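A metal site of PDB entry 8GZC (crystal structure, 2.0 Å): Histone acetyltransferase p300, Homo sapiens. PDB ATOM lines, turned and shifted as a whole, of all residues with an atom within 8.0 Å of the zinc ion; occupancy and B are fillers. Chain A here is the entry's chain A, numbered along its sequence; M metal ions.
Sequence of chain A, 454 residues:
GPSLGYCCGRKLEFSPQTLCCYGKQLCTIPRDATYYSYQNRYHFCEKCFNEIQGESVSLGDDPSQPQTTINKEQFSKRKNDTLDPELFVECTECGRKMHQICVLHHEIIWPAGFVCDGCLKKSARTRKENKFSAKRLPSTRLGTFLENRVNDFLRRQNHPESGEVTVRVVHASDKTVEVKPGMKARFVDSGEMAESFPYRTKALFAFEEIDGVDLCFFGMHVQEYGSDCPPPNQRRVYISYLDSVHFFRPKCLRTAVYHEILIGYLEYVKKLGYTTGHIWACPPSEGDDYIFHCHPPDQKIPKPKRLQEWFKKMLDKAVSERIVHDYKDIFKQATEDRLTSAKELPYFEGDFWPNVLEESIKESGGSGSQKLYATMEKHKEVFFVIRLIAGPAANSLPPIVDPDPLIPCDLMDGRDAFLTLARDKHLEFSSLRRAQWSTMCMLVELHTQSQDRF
SG of Cys 119 sits close to OE1 of Glu 93, 3.6 Å away. N of Glu 93 sits close to SG of Cys 91 (3.6 Å). The side-chain sulfur (SG) of Cys 94 sits close to the backbone NH (N) of Arg 96, at 3.5 Å. The side-chain sulfur (SG) of Cys 116 lies close to the backbone NH (N) of Gly 118. The backbone NH (N) of Cys 91 lies within hydrogen-bond range of the backbone carbonyl oxygen (O) of Arg 96, 3.0 Å away. The guanidinium group (NH2) of Arg 125 sits at hydrogen-bond distance from the backbone carbonyl oxygen (O) of Cys 119.
Of the 17 residues printed, 4 come within 4 Å of the zinc ion.
The zinc ion is bound by SG of Cys 91, SG of Cys 116, SG of Cys 119 and SG of Cys 94. The zinc ion has four donor atoms within binding distance.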
ATOM      1  N   GLU A  90     -28.231  31.535  26.101  1.00  0.00           N
ATOM      2  CA  GLU A  90     -28.410  30.237  26.737  1.00  0.00           C
ATOM      3  C   GLU A  90     -27.105  29.460  26.664  1.00  0.00           C
ATOM      4  O   GLU A  90     -26.501  29.355  25.588  1.00  0.00           O
ATOM      5  CB  GLU A  90     -29.537  29.453  26.063  1.00  0.00           C
ATOM      6  CG  GLU A  90     -29.837  28.118  26.699  1.00  0.00           C
ATOM      7  CD  GLU A  90     -31.050  27.456  26.081  1.00  0.00           C
ATOM      8  OE1 GLU A  90     -31.023  27.196  24.860  1.00  0.00           O
ATOM      9  OE2 GLU A  90     -32.031  27.205  26.811  1.00  0.00           O
ATOM     10  N   CYS A  91     -26.666  28.929  27.795  1.00  0.00           N
ATOM     11  CA  CYS A  91     -25.484  28.082  27.821  1.00  0.00           C
ATOM     12  C   CYS A  91     -25.766  26.809  27.041  1.00  0.00           C
ATOM     13  O   CYS A  91     -26.765  26.120  27.285  1.00  0.00           O
ATOM     14  CB  CYS A  91     -25.082  27.750  29.263  1.00  0.00           C
ATOM     15  SG  CYS A  91     -23.614  26.698  29.408  1.00  0.00           S
ATOM     16  N   THR A  92     -24.874  26.476  26.102  1.00  0.00           N
ATOM     17  CA  THR A  92     -25.100  25.333  25.228  1.00  0.00           C
ATOM     18  C   THR A  92     -25.050  24.004  25.975  1.00  0.00           C
ATOM     19  O   THR A  92     -25.318  22.964  25.368  1.00  0.00           O
ATOM     20  CB  THR A  92     -24.072  25.325  24.092  1.00  0.00           C
ATOM     21  OG1 THR A  92     -22.753  25.497  24.640  1.00  0.00           O
ATOM     22  CG2 THR A  92     -24.363  26.457  23.116  1.00  0.00           C
ATOM     23  N   GLU A  93     -24.698  24.004  27.265  1.00  0.00           N
ATOM     24  CA  GLU A  93     -24.599  22.767  28.035  1.00  0.00           C
ATOM     25  C   GLU A  93     -25.636  22.686  29.160  1.00  0.00           C
ATOM     26  O   GLU A  93     -26.454  21.762  29.157  1.00  0.00           O
ATOM     27  CB  GLU A  93     -23.180  22.633  28.575  1.00  0.00           C
ATOM     28  CG  GLU A  93     -22.115  22.720  27.491  1.00  0.00           C
ATOM     29  CD  GLU A  93     -20.701  22.660  28.035  1.00  0.00           C
ATOM     30  OE1 GLU A  93     -20.534  22.552  29.259  1.00  0.00           O
ATOM     31  OE2 GLU A  93     -19.753  22.735  27.224  1.00  0.00           O
ATOM     32  N   CYS A  94     -25.645  23.646  30.085  1.00  0.00           N
ATOM     33  CA  CYS A  94     -26.598  23.568  31.191  1.00  0.00           C
ATOM     34  C   CYS A  94     -27.937  24.216  30.864  1.00  0.00           C
ATOM     35  O   CYS A  94     -28.892  24.046  31.630  1.00  0.00           O
ATOM     36  CB  CYS A  94     -26.003  24.217  32.451  1.00  0.00           C
ATOM     37  SG  CYS A  94     -25.732  25.988  32.340  1.00  0.00           S
ATOM     38  N   GLY A  95     -28.028  24.944  29.758  1.00  0.00           N
ATOM     39  CA  GLY A  95     -29.277  25.587  29.402  1.00  0.00           C
ATOM     40  C   GLY A  95     -29.631  26.789  30.242  1.00  0.00           C
ATOM     41  O   GLY A  95     -30.755  27.289  30.144  1.00  0.00           O
ATOM     42  N   ARG A  96     -28.714  27.266  31.086  1.00  0.00           N
ATOM     43  CA  ARG A  96     -28.982  28.439  31.901  1.00  0.00           C
ATOM     44  C   ARG A  96     -29.077  29.679  31.026  1.00  0.00           C
ATOM     45  O   ARG A  96     -28.288  29.878  30.103  1.00  0.00           O
ATOM     46  CB  ARG A  96     -27.892  28.626  32.952  1.00  0.00           C
ATOM     47  N   LYS A  97     -30.070  30.521  31.318  1.00  0.00           N
ATOM     48  CA  LYS A  97     -30.313  31.744  30.558  1.00  0.00           C
ATOM     49  C   LYS A  97     -29.615  32.909  31.250  1.00  0.00           C
ATOM     50  O   LYS A  97     -29.768  33.101  32.451  1.00  0.00           O
ATOM     51  CB  LYS A  97     -31.818  32.012  30.438  1.00  0.00           C
ATOM     52  N   MET A  98     -28.862  33.692  30.479  1.00  0.00           N
ATOM     53  CA  MET A  98     -28.037  34.760  31.037  1.00  0.00           C
ATOM     54  C   MET A  98     -28.130  36.010  30.175  1.00  0.00           C
ATOM     55  O   MET A  98     -28.073  35.924  28.950  1.00  0.00           O
ATOM     56  CB  MET A  98     -26.566  34.319  31.139  1.00  0.00           C
ATOM     57  CG  MET A  98     -26.301  33.138  32.076  1.00  0.00           C
ATOM     58  SD  MET A  98     -25.945  33.633  33.775  1.00  0.00           S
ATOM     59  CE  MET A  98     -27.612  33.902  34.322  1.00  0.00           C
ATOM     60  N   PHE A 114     -22.412  29.849  23.354  1.00  0.00           N
ATOM     61  CA  PHE A 114     -22.176  30.348  24.702  1.00  0.00           C
ATOM     62  C   PHE A 114     -22.059  29.190  25.687  1.00  0.00           C
ATOM     63  O   PHE A 114     -22.927  28.307  25.722  1.00  0.00           O
ATOM     64  CB  PHE A 114     -23.290  31.287  25.142  1.00  0.00           C
ATOM     65  CG  PHE A 114     -23.248  31.644  26.605  1.00  0.00           C
ATOM     66  CD1 PHE A 114     -22.100  32.169  27.163  1.00  0.00           C
ATOM     67  CD2 PHE A 114     -24.354  31.442  27.417  1.00  0.00           C
ATOM     68  CE1 PHE A 114     -22.046  32.489  28.505  1.00  0.00           C
ATOM     69  CE2 PHE A 114     -24.313  31.769  28.756  1.00  0.00           C
ATOM     70  CZ  PHE A 114     -23.158  32.287  29.304  1.00  0.00           C
ATOM     71  N   VAL A 115     -20.991  29.193  26.477  1.00  0.00           N
ATOM     72  CA  VAL A 115     -20.792  28.239  27.563  1.00  0.00           C
ATOM     73  C   VAL A 115     -20.618  29.046  28.845  1.00  0.00           C
ATOM     74  O   VAL A 115     -19.683  29.841  28.958  1.00  0.00           O
ATOM     75  CB  VAL A 115     -19.582  27.336  27.318  1.00  0.00           C
ATOM     76  CG1 VAL A 115     -19.403  26.346  28.464  1.00  0.00           C
ATOM     77  CG2 VAL A 115     -19.731  26.598  25.994  1.00  0.00           C
ATOM     78  N   CYS A 116     -21.517  28.832  29.809  1.00  0.00           N
ATOM     79  CA  CYS A 116     -21.503  29.604  31.039  1.00  0.00           C
ATOM     80  C   CYS A 116     -20.225  29.321  31.835  1.00  0.00           C
ATOM     81  O   CYS A 116     -19.515  28.341  31.591  1.00  0.00           O
ATOM     82  CB  CYS A 116     -22.732  29.308  31.880  1.00  0.00           C
ATOM     83  SG  CYS A 116     -22.573  27.892  32.999  1.00  0.00           S
ATOM     84  N   ASP A 117     -19.937  30.198  32.793  1.00  0.00           N
ATOM     85  CA  ASP A 117     -18.718  30.067  33.575  1.00  0.00           C
ATOM     86  C   ASP A 117     -18.758  28.836  34.477  1.00  0.00           C
ATOM     87  O   ASP A 117     -17.705  28.234  34.745  1.00  0.00           O
ATOM     88  CB  ASP A 117     -18.486  31.325  34.412  1.00  0.00           C
ATOM     89  CG  ASP A 117     -17.477  32.268  33.771  1.00  0.00           C
ATOM     90  OD1 ASP A 117     -16.785  31.837  32.827  1.00  0.00           O
ATOM     91  OD2 ASP A 117     -17.390  33.429  34.205  1.00  0.00           O
ATOM     92  N   GLY A 118     -19.932  28.441  34.951  1.00  0.00           N
ATOM     93  CA  GLY A 118     -20.031  27.232  35.746  1.00  0.00           C
ATOM     94  C   GLY A 118     -19.613  25.993  34.980  1.00  0.00           C
ATOM     95  O   GLY A 118     -18.867  25.157  35.491  1.00  0.00           O
ATOM     96  N   CYS A 119     -20.062  25.874  33.732  1.00  0.00           N
ATOM     97  CA  CYS A 119     -19.659  24.756  32.892  1.00  0.00           C
ATOM     98  C   CYS A 119     -18.185  24.848  32.499  1.00  0.00           C
ATOM     99  O   CYS A 119     -17.590  23.825  32.150  1.00  0.00           O
ATOM    100  CB  CYS A 119     -20.530  24.701  31.635  1.00  0.00           C
ATOM    101  SG  CYS A 119     -22.255  24.261  31.943  1.00  0.00           S
ATOM    102  N   LEU A 120     -17.589  26.036  32.551  1.00  0.00           N
ATOM    103  CA  LEU A 120     -16.184  26.183  32.204  1.00  0.00           C
ATOM    104  C   LEU A 120     -15.276  25.830  33.380  1.00  0.00           C
ATOM    105  O   LEU A 120     -14.310  25.081  33.228  1.00  0.00           O
ATOM    106  CB  LEU A 120     -15.905  27.610  31.721  1.00  0.00           C
ATOM    107  CG  LEU A 120     -16.373  27.946  30.304  1.00  0.00           C
ATOM    108  CD1 LEU A 120     -16.159  29.423  30.016  1.00  0.00           C
ATOM    109  CD2 LEU A 120     -15.669  27.086  29.278  1.00  0.00           C
ATOM    110  N   ARG A 125     -11.979  24.420  31.962  1.00  0.00           N
ATOM    111  CA  ARG A 125     -11.892  25.027  30.635  1.00  0.00           C
ATOM    112  C   ARG A 125     -11.930  26.542  30.762  1.00  0.00           C
ATOM    113  O   ARG A 125     -12.359  27.099  31.787  1.00  0.00           O
ATOM    114  CB  ARG A 125     -13.030  24.546  29.727  1.00  0.00           C
ATOM    115  CG  ARG A 125     -12.621  23.483  28.722  1.00  0.00           C
ATOM    116  CD  ARG A 125     -13.829  22.897  28.016  1.00  0.00           C
ATOM    117  NE  ARG A 125     -14.981  22.776  28.908  1.00  0.00           N
ATOM    118  CZ  ARG A 125     -16.244  22.856  28.517  1.00  0.00           C
ATOM    119  NH1 ARG A 125     -16.568  23.070  27.251  1.00  0.00           N
ATOM    120  NH2 ARG A 125     -17.208  22.733  29.418  1.00  0.00           N
HETATM  121 ZN    ZN M   1     -23.502  26.212  31.680  1.00  0.00          ZN
